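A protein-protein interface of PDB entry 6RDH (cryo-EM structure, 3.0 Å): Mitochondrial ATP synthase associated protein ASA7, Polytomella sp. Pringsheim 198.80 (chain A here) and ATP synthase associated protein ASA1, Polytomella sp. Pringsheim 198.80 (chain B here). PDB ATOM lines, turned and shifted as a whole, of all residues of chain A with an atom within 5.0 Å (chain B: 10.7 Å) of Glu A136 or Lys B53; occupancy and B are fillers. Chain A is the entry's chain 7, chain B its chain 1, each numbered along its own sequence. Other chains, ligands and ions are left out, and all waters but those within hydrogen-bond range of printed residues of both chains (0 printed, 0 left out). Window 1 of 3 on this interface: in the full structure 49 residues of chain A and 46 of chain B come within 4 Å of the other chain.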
ATOM      1  N   TRP A 107       2.855   4.259  20.753  1.00  0.00           N
ATOM      2  CA  TRP A 107       3.537   5.253  21.561  1.00  0.00           C
ATOM      3  C   TRP A 107       5.008   5.276  21.167  1.00  0.00           C
ATOM      4  O   TRP A 107       5.586   4.222  20.906  1.00  0.00           O
ATOM      5  CB  TRP A 107       3.410   4.885  23.017  1.00  0.00           C
ATOM      6  CG  TRP A 107       3.541   5.969  23.985  1.00  0.00           C
ATOM      7  CD1 TRP A 107       4.674   6.397  24.585  1.00  0.00           C
ATOM      8  CD2 TRP A 107       2.474   6.687  24.584  1.00  0.00           C
ATOM      9  NE1 TRP A 107       4.390   7.390  25.480  1.00  0.00           N
ATOM     10  CE2 TRP A 107       3.036   7.579  25.501  1.00  0.00           C
ATOM     11  CE3 TRP A 107       1.092   6.675  24.415  1.00  0.00           C
ATOM     12  CZ2 TRP A 107       2.269   8.450  26.244  1.00  0.00           C
ATOM     13  CZ3 TRP A 107       0.335   7.530  25.153  1.00  0.00           C
ATOM     14  CH2 TRP A 107       0.922   8.405  26.057  1.00  0.00           C
ATOM     15  N   ASP A 132       8.645  12.563  33.458  1.00  0.00           N
ATOM     16  CA  ASP A 132       7.272  12.399  33.915  1.00  0.00           C
ATOM     17  C   ASP A 132       6.389  11.771  32.846  1.00  0.00           C
ATOM     18  O   ASP A 132       5.479  11.008  33.174  1.00  0.00           O
ATOM     19  CB  ASP A 132       6.691  13.744  34.332  1.00  0.00           C
ATOM     20  CG  ASP A 132       7.073  14.129  35.736  1.00  0.00           C
ATOM     21  OD1 ASP A 132       7.432  13.229  36.522  1.00  0.00           O
ATOM     22  OD2 ASP A 132       7.006  15.331  36.058  1.00  0.00           O
ATOM     23  N   ALA A 133       6.647  12.065  31.573  1.00  0.00           N
ATOM     24  CA  ALA A 133       5.878  11.444  30.502  1.00  0.00           C
ATOM     25  C   ALA A 133       6.194   9.960  30.376  1.00  0.00           C
ATOM     26  O   ALA A 133       5.303   9.153  30.081  1.00  0.00           O
ATOM     27  CB  ALA A 133       6.153  12.163  29.187  1.00  0.00           C
ATOM     28  N   ALA A 134       7.447   9.578  30.618  1.00  0.00           N
ATOM     29  CA  ALA A 134       7.793   8.158  30.622  1.00  0.00           C
ATOM     30  C   ALA A 134       7.130   7.423  31.786  1.00  0.00           C
ATOM     31  O   ALA A 134       6.595   6.318  31.614  1.00  0.00           O
ATOM     32  CB  ALA A 134       9.306   7.991  30.671  1.00  0.00           C
ATOM     33  N   ASP A 135       7.143   8.031  32.977  1.00  0.00           N
ATOM     34  CA  ASP A 135       6.461   7.438  34.129  1.00  0.00           C
ATOM     35  C   ASP A 135       4.956   7.338  33.905  1.00  0.00           C
ATOM     36  O   ASP A 135       4.310   6.373  34.338  1.00  0.00           O
ATOM     37  CB  ASP A 135       6.752   8.262  35.377  1.00  0.00           C
ATOM     38  CG  ASP A 135       7.846   7.663  36.228  1.00  0.00           C
ATOM     39  OD1 ASP A 135       8.328   6.561  35.892  1.00  0.00           O
ATOM     40  OD2 ASP A 135       8.227   8.294  37.235  1.00  0.00           O
ATOM     41  N   GLU A 136       4.391   8.310  33.194  1.00  0.00           N
ATOM     42  CA  GLU A 136       2.976   8.286  32.858  1.00  0.00           C
ATOM     43  C   GLU A 136       2.641   7.153  31.903  1.00  0.00           C
ATOM     44  O   GLU A 136       1.611   6.489  32.074  1.00  0.00           O
ATOM     45  CB  GLU A 136       2.593   9.623  32.253  1.00  0.00           C
ATOM     46  CG  GLU A 136       1.177   9.748  31.813  1.00  0.00           C
ATOM     47  CD  GLU A 136       1.032  10.857  30.805  1.00  0.00           C
ATOM     48  OE1 GLU A 136       1.604  10.732  29.702  1.00  0.00           O
ATOM     49  OE2 GLU A 136       0.374  11.865  31.119  1.00  0.00           O
ATOM     50  N   TYR A 137       3.487   6.916  30.893  1.00  0.00           N
ATOM     51  CA  TYR A 137       3.256   5.778  30.002  1.00  0.00           C
ATOM     52  C   TYR A 137       3.341   4.460  30.748  1.00  0.00           C
ATOM     53  O   TYR A 137       2.588   3.532  30.444  1.00  0.00           O
ATOM     54  CB  TYR A 137       4.250   5.754  28.850  1.00  0.00           C
ATOM     55  CG  TYR A 137       4.132   4.512  27.981  1.00  0.00           C
ATOM     56  CD1 TYR A 137       3.140   4.413  27.033  1.00  0.00           C
ATOM     57  CD2 TYR A 137       5.006   3.439  28.117  1.00  0.00           C
ATOM     58  CE1 TYR A 137       3.026   3.301  26.242  1.00  0.00           C
ATOM     59  CE2 TYR A 137       4.890   2.324  27.339  1.00  0.00           C
ATOM     60  CZ  TYR A 137       3.902   2.263  26.402  1.00  0.00           C
ATOM     61  OH  TYR A 137       3.777   1.157  25.614  1.00  0.00           O
ATOM     62  N   TYR A 138       4.281   4.333  31.687  1.00  0.00           N
ATOM     63  CA  TYR A 138       4.350   3.093  32.459  1.00  0.00           C
ATOM     64  C   TYR A 138       3.115   2.902  33.318  1.00  0.00           C
ATOM     65  O   TYR A 138       2.665   1.770  33.498  1.00  0.00           O
ATOM     66  CB  TYR A 138       5.590   3.067  33.336  1.00  0.00           C
ATOM     67  CG  TYR A 138       6.849   2.858  32.564  1.00  0.00           C
ATOM     68  CD1 TYR A 138       6.957   1.837  31.646  1.00  0.00           C
ATOM     69  CD2 TYR A 138       7.920   3.706  32.733  1.00  0.00           C
ATOM     70  CE1 TYR A 138       8.105   1.662  30.933  1.00  0.00           C
ATOM     71  CE2 TYR A 138       9.062   3.543  32.021  1.00  0.00           C
ATOM     72  CZ  TYR A 138       9.150   2.523  31.128  1.00  0.00           C
ATOM     73  OH  TYR A 138      10.309   2.380  30.432  1.00  0.00           O
ATOM     74  N   LYS A 139       2.527   3.994  33.808  1.00  0.00           N
ATOM     75  CA  LYS A 139       1.260   3.893  34.530  1.00  0.00           C
ATOM     76  C   LYS A 139       0.139   3.401  33.625  1.00  0.00           C
ATOM     77  O   LYS A 139      -0.601   2.474  33.982  1.00  0.00           O
ATOM     78  CB  LYS A 139       0.897   5.247  35.127  1.00  0.00           C
ATOM     79  CG  LYS A 139      -0.280   5.210  36.053  1.00  0.00           C
ATOM     80  CD  LYS A 139      -0.763   6.608  36.347  1.00  0.00           C
ATOM     81  CE  LYS A 139      -1.568   7.161  35.197  1.00  0.00           C
ATOM     82  NZ  LYS A 139      -2.886   6.494  35.084  1.00  0.00           N
ATOM     83  N   LEU A 140       0.017   4.004  32.438  1.00  0.00           N
ATOM     84  CA  LEU A 140      -1.055   3.647  31.509  1.00  0.00           C
ATOM     85  C   LEU A 140      -0.914   2.218  31.014  1.00  0.00           C
ATOM     86  O   LEU A 140      -1.908   1.497  30.891  1.00  0.00           O
ATOM     87  CB  LEU A 140      -1.070   4.605  30.323  1.00  0.00           C
ATOM     88  CG  LEU A 140      -1.291   6.080  30.626  1.00  0.00           C
ATOM     89  CD1 LEU A 140      -1.301   6.879  29.351  1.00  0.00           C
ATOM     90  CD2 LEU A 140      -2.558   6.287  31.404  1.00  0.00           C
ATOM     91  N   ASN B  45     -13.520  10.944  27.158  1.00  0.00           N
ATOM     92  CA  ASN B  45     -12.431  11.587  26.446  1.00  0.00           C
ATOM     93  C   ASN B  45     -11.113  10.846  26.618  1.00  0.00           C
ATOM     94  O   ASN B  45     -10.055  11.417  26.345  1.00  0.00           O
ATOM     95  CB  ASN B  45     -12.291  13.036  26.911  1.00  0.00           C
ATOM     96  CG  ASN B  45     -11.899  13.970  25.792  1.00  0.00           C
ATOM     97  OD1 ASN B  45     -12.364  13.834  24.664  1.00  0.00           O
ATOM     98  ND2 ASN B  45     -11.032  14.926  26.097  1.00  0.00           N
ATOM     99  N   LEU B  46     -11.158   9.582  27.049  1.00  0.00           N
ATOM    100  CA  LEU B  46      -9.934   8.852  27.361  1.00  0.00           C
ATOM    101  C   LEU B  46      -9.136   8.509  26.116  1.00  0.00           C
ATOM    102  O   LEU B  46      -7.906   8.477  26.170  1.00  0.00           O
ATOM    103  CB  LEU B  46     -10.250   7.569  28.111  1.00  0.00           C
ATOM    104  CG  LEU B  46      -9.073   6.913  28.822  1.00  0.00           C
ATOM    105  CD1 LEU B  46      -8.930   7.484  30.215  1.00  0.00           C
ATOM    106  CD2 LEU B  46      -9.221   5.417  28.851  1.00  0.00           C
ATOM    107  N   VAL B  47      -9.800   8.240  24.995  1.00  0.00           N
ATOM    108  CA  VAL B  47      -9.064   8.009  23.759  1.00  0.00           C
ATOM    109  C   VAL B  47      -8.436   9.305  23.277  1.00  0.00           C
ATOM    110  O   VAL B  47      -7.284   9.329  22.827  1.00  0.00           O
ATOM    111  CB  VAL B  47      -9.988   7.400  22.694  1.00  0.00           C
ATOM    112  CG1 VAL B  47      -9.225   7.120  21.416  1.00  0.00           C
ATOM    113  CG2 VAL B  47     -10.636   6.147  23.223  1.00  0.00           C
ATOM    114  N   ASN B  48      -9.157  10.414  23.425  1.00  0.00           N
ATOM    115  CA  ASN B  48      -8.620  11.703  23.017  1.00  0.00           C
ATOM    116  C   ASN B  48      -7.530  12.169  23.969  1.00  0.00           C
ATOM    117  O   ASN B  48      -6.526  12.736  23.532  1.00  0.00           O
ATOM    118  CB  ASN B  48      -9.744  12.732  22.936  1.00  0.00           C
ATOM    119  CG  ASN B  48      -9.299  14.028  22.309  1.00  0.00           C
ATOM    120  OD1 ASN B  48      -8.880  14.954  22.999  1.00  0.00           O
ATOM    121  ND2 ASN B  48      -9.399  14.106  20.988  1.00  0.00           N
ATOM    122  N   GLU B  49      -7.682  11.896  25.267  1.00  0.00           N
ATOM    123  CA  GLU B  49      -6.628  12.241  26.216  1.00  0.00           C
ATOM    124  C   GLU B  49      -5.397  11.368  26.043  1.00  0.00           C
ATOM    125  O   GLU B  49      -4.280  11.841  26.247  1.00  0.00           O
ATOM    126  CB  GLU B  49      -7.139  12.136  27.644  1.00  0.00           C
ATOM    127  CG  GLU B  49      -7.882  13.359  28.099  1.00  0.00           C
ATOM    128  CD  GLU B  49      -8.204  13.309  29.570  1.00  0.00           C
ATOM    129  OE1 GLU B  49      -8.039  12.227  30.170  1.00  0.00           O
ATOM    130  OE2 GLU B  49      -8.618  14.347  30.126  1.00  0.00           O
ATOM    131  N   TRP B  50      -5.562  10.111  25.650  1.00  0.00           N
ATOM    132  CA  TRP B  50      -4.382   9.288  25.440  1.00  0.00           C
ATOM    133  C   TRP B  50      -3.693   9.624  24.127  1.00  0.00           C
ATOM    134  O   TRP B  50      -2.463   9.533  24.041  1.00  0.00           O
ATOM    135  CB  TRP B  50      -4.745   7.813  25.496  1.00  0.00           C
ATOM    136  CG  TRP B  50      -4.946   7.303  26.873  1.00  0.00           C
ATOM    137  CD1 TRP B  50      -5.182   8.037  27.990  1.00  0.00           C
ATOM    138  CD2 TRP B  50      -4.938   5.940  27.285  1.00  0.00           C
ATOM    139  NE1 TRP B  50      -5.319   7.219  29.074  1.00  0.00           N
ATOM    140  CE2 TRP B  50      -5.172   5.922  28.667  1.00  0.00           C
ATOM    141  CE3 TRP B  50      -4.747   4.731  26.621  1.00  0.00           C
ATOM    142  CZ2 TRP B  50      -5.227   4.745  29.392  1.00  0.00           C
ATOM    143  CZ3 TRP B  50      -4.805   3.569  27.342  1.00  0.00           C
ATOM    144  CH2 TRP B  50      -5.042   3.580  28.712  1.00  0.00           C
ATOM    145  N   ASN B  51      -4.447  10.060  23.116  1.00  0.00           N
ATOM    146  CA  ASN B  51      -3.815  10.614  21.924  1.00  0.00           C
ATOM    147  C   ASN B  51      -3.107  11.927  22.230  1.00  0.00           C
ATOM    148  O   ASN B  51      -2.047  12.200  21.660  1.00  0.00           O
ATOM    149  CB  ASN B  51      -4.848  10.816  20.820  1.00  0.00           C
ATOM    150  CG  ASN B  51      -5.165   9.538  20.080  1.00  0.00           C
ATOM    151  OD1 ASN B  51      -4.324   8.652  19.965  1.00  0.00           O
ATOM    152  ND2 ASN B  51      -6.383   9.439  19.568  1.00  0.00           N
ATOM    153  N   ASN B  52      -3.662  12.729  23.143  1.00  0.00           N
ATOM    154  CA  ASN B  52      -2.997  13.952  23.581  1.00  0.00           C
ATOM    155  C   ASN B  52      -1.705  13.655  24.324  1.00  0.00           C
ATOM    156  O   ASN B  52      -0.712  14.362  24.150  1.00  0.00           O
ATOM    157  CB  ASN B  52      -3.921  14.761  24.479  1.00  0.00           C
ATOM    158  CG  ASN B  52      -4.945  15.520  23.708  1.00  0.00           C
ATOM    159  OD1 ASN B  52      -5.015  15.418  22.488  1.00  0.00           O
ATOM    160  ND2 ASN B  52      -5.756  16.290  24.411  1.00  0.00           N
ATOM    161  N   LYS B  53      -1.711  12.631  25.171  1.00  0.00           N
ATOM    162  CA  LYS B  53      -0.509  12.269  25.904  1.00  0.00           C
ATOM    163  C   LYS B  53       0.556  11.710  24.974  1.00  0.00           C
ATOM    164  O   LYS B  53       1.747  11.995  25.149  1.00  0.00           O
ATOM    165  CB  LYS B  53      -0.855  11.271  26.997  1.00  0.00           C
ATOM    166  CG  LYS B  53      -1.568  11.868  28.170  1.00  0.00           C
ATOM    167  CD  LYS B  53      -2.093  10.799  29.089  1.00  0.00           C
ATOM    168  CE  LYS B  53      -2.806  11.421  30.264  1.00  0.00           C
ATOM    169  NZ  LYS B  53      -3.233  10.399  31.249  1.00  0.00           N
ATOM    170  N   LYS B  54       0.147  10.948  23.956  1.00  0.00           N
ATOM    171  CA  LYS B  54       1.103  10.475  22.961  1.00  0.00           C
ATOM    172  C   LYS B  54       1.670  11.627  22.145  1.00  0.00           C
ATOM    173  O   LYS B  54       2.869  11.649  21.846  1.00  0.00           O
ATOM    174  CB  LYS B  54       0.442   9.455  22.041  1.00  0.00           C
ATOM    175  CG  LYS B  54       1.373   8.841  21.029  1.00  0.00           C
ATOM    176  CD  LYS B  54       0.632   7.920  20.098  1.00  0.00           C
ATOM    177  CE  LYS B  54      -0.282   8.699  19.193  1.00  0.00           C
ATOM    178  NZ  LYS B  54      -0.959   7.834  18.199  1.00  0.00           N
ATOM    179  N   GLN B  55       0.836  12.615  21.817  1.00  0.00           N
ATOM    180  CA  GLN B  55       1.318  13.764  21.057  1.00  0.00           C
ATOM    181  C   GLN B  55       2.227  14.647  21.897  1.00  0.00           C
ATOM    182  O   GLN B  55       3.197  15.206  21.382  1.00  0.00           O
ATOM    183  CB  GLN B  55       0.142  14.573  20.518  1.00  0.00           C
ATOM    184  CG  GLN B  55       0.526  15.600  19.473  1.00  0.00           C
ATOM    185  CD  GLN B  55       1.124  14.974  18.231  1.00  0.00           C
ATOM    186  OE1 GLN B  55       0.711  13.899  17.798  1.00  0.00           O
ATOM    187  NE2 GLN B  55       2.107  15.648  17.648  1.00  0.00           N
ATOM    188  N   ALA B  56       1.947  14.767  23.193  1.00  0.00           N
ATOM    189  CA  ALA B  56       2.811  15.558  24.058  1.00  0.00           C
ATOM    190  C   ALA B  56       4.156  14.884  24.259  1.00  0.00           C
ATOM    191  O   ALA B  56       5.190  15.554  24.269  1.00  0.00           O
ATOM    192  CB  ALA B  56       2.137  15.802  25.403  1.00  0.00           C
ATOM    193  N   THR B  57       4.167  13.560  24.395  1.00  0.00           N
ATOM    194  CA  THR B  57       5.435  12.854  24.526  1.00  0.00           C
ATOM    195  C   THR B  57       6.221  12.886  23.223  1.00  0.00           C
ATOM    196  O   THR B  57       7.456  12.963  23.234  1.00  0.00           O
ATOM    197  CB  THR B  57       5.178  11.422  24.968  1.00  0.00           C
ATOM    198  OG1 THR B  57       4.227  11.438  26.036  1.00  0.00           O
ATOM    199  CG2 THR B  57       6.436  10.783  25.471  1.00  0.00           C
ATOM    200  N   GLU B  58       5.530  12.883  22.084  1.00  0.00           N
ATOM    201  CA  GLU B  58       6.244  13.003  20.820  1.00  0.00           C
ATOM    202  C   GLU B  58       6.771  14.413  20.604  1.00  0.00           C
ATOM    203  O   GLU B  58       7.848  14.587  20.027  1.00  0.00           O
ATOM    204  CB  GLU B  58       5.343  12.590  19.669  1.00  0.00           C
ATOM    205  CG  GLU B  58       6.098  12.011  18.507  1.00  0.00           C
ATOM    206  CD  GLU B  58       5.241  11.107  17.652  1.00  0.00           C
ATOM    207  OE1 GLU B  58       4.031  10.984  17.933  1.00  0.00           O
ATOM    208  OE2 GLU B  58       5.783  10.517  16.695  1.00  0.00           O
ATOM    209  N   ASN B  59       6.046  15.428  21.076  1.00  0.00           N
ATOM    210  CA  ASN B  59       6.562  16.790  21.025  1.00  0.00           C
ATOM    211  C   ASN B  59       7.754  16.959  21.951  1.00  0.00           C
ATOM    212  O   ASN B  59       8.687  17.695  21.632  1.00  0.00           O
ATOM    213  CB  ASN B  59       5.471  17.785  21.395  1.00  0.00           C
ATOM    214  CG  ASN B  59       4.468  17.969  20.302  1.00  0.00           C
ATOM    215  OD1 ASN B  59       4.699  17.576  19.165  1.00  0.00           O
ATOM    216  ND2 ASN B  59       3.340  18.574  20.636  1.00  0.00           N
ATOM    217  N   LEU B  60       7.744  16.278  23.095  1.00  0.00           N
ATOM    218  CA  LEU B  60       8.889  16.323  23.994  1.00  0.00           C
ATOM    219  C   LEU B  60      10.095  15.642  23.379  1.00  0.00           C
ATOM    220  O   LEU B  60      11.220  16.105  23.554  1.00  0.00           O
ATOM    221  CB  LEU B  60       8.540  15.674  25.327  1.00  0.00           C
ATOM    222  CG  LEU B  60       7.783  16.549  26.311  1.00  0.00           C
ATOM    223  CD1 LEU B  60       7.158  15.696  27.379  1.00  0.00           C
ATOM    224  CD2 LEU B  60       8.729  17.545  26.925  1.00  0.00           C
ATOM    225  N   MET B  61       9.887  14.557  22.640  1.00  0.00           N
ATOM    226  CA  MET B  61      11.021  13.914  21.987  1.00  0.00           C
ATOM    227  C   MET B  61      11.547  14.744  20.827  1.00  0.00           C
ATOM    228  O   MET B  61      12.761  14.790  20.596  1.00  0.00           O
ATOM    229  CB  MET B  61      10.638  12.524  21.512  1.00  0.00           C
ATOM    230  CG  MET B  61      10.666  11.528  22.610  1.00  0.00           C
ATOM    231  SD  MET B  61      10.371   9.896  22.015  1.00  0.00           S
ATOM    232  CE  MET B  61       8.956   9.584  23.037  1.00  0.00           C
ATOM    233  N   VAL B 151       7.324   1.870  20.945  1.00  0.00           N
ATOM    234  CA  VAL B 151       7.642   1.038  22.098  1.00  0.00           C
ATOM    235  C   VAL B 151       7.282  -0.404  21.784  1.00  0.00           C
ATOM    236  O   VAL B 151       6.179  -0.695  21.307  1.00  0.00           O
ATOM    237  CB  VAL B 151       6.904   1.523  23.350  1.00  0.00           C
ATOM    238  CG1 VAL B 151       7.424   0.808  24.551  1.00  0.00           C
ATOM    239  CG2 VAL B 151       7.088   2.990  23.542  1.00  0.00           C
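Printed residues of chain B that touch a printed residue of chain A: Trp B50, Lys B53, Lys B54, Thr B57 and Val B151.
Among the printed residues, 9 pairs touch across the chains.
Among the printed residues, Asp or Glu carboxylates within 4 Å of a Lys or Arg side-chain nitrogen of the other chain: Glu A136 with Lys B53 (3.9 Å).
The backbone carbonyl oxygen of Lys B53 is in hydrogen-bond range of the side-chain hydroxyl of Thr B57, 2.7 Å away.
Of the printed residues of chain A, Lys B53 touches Trp A107 and Glu A136.
Of chain B, only Thr B57 (3.8 Å) comes within 4 Å of Ala A133.
No residue of chain B comes within 4 Å of Ala A134.
No residue of chain B comes within 4 Å of Asp A135.
Of the printed residues of chain B, Trp A107 touches Trp B50, Lys B53, Lys B54, Thr B57 and Val B151.
Printed residues of chain B within 4 Å of Tyr A137: Val B151.
Of the printed residues of chain B, Leu A140 touches Trp B50.
The nearest residue of chain B that does not touch Glu A136 is Thr B57 (4.6 Å).
The nearest printed residue of chain A that does not touch Lys B53 is Leu A140 (4.01 Å).
The nearest printed residue of chain A that does not touch Lys B54 is Glu A136 (5.9 Å).
Among the printed residues, merely in contact across the chains: Trp A107 with Lys B54, Trp A107 with Lys B53, Trp A107 with Thr B57, Trp A107 with Trp B50, Leu A140 with Trp B50, Ala A133 with Thr B57 and Tyr A137 with Val B151.
The side-chain amino group (NZ) of Lys B53 is in salt-bridge range of the side-chain carboxylate (OE2) of Glu A136 (3.9 Å).
The backbone NH (N) of Val B151 lies within hydrogen-bond range of the backbone carbonyl oxygen (O) of Trp A107, 2.9 Å away.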
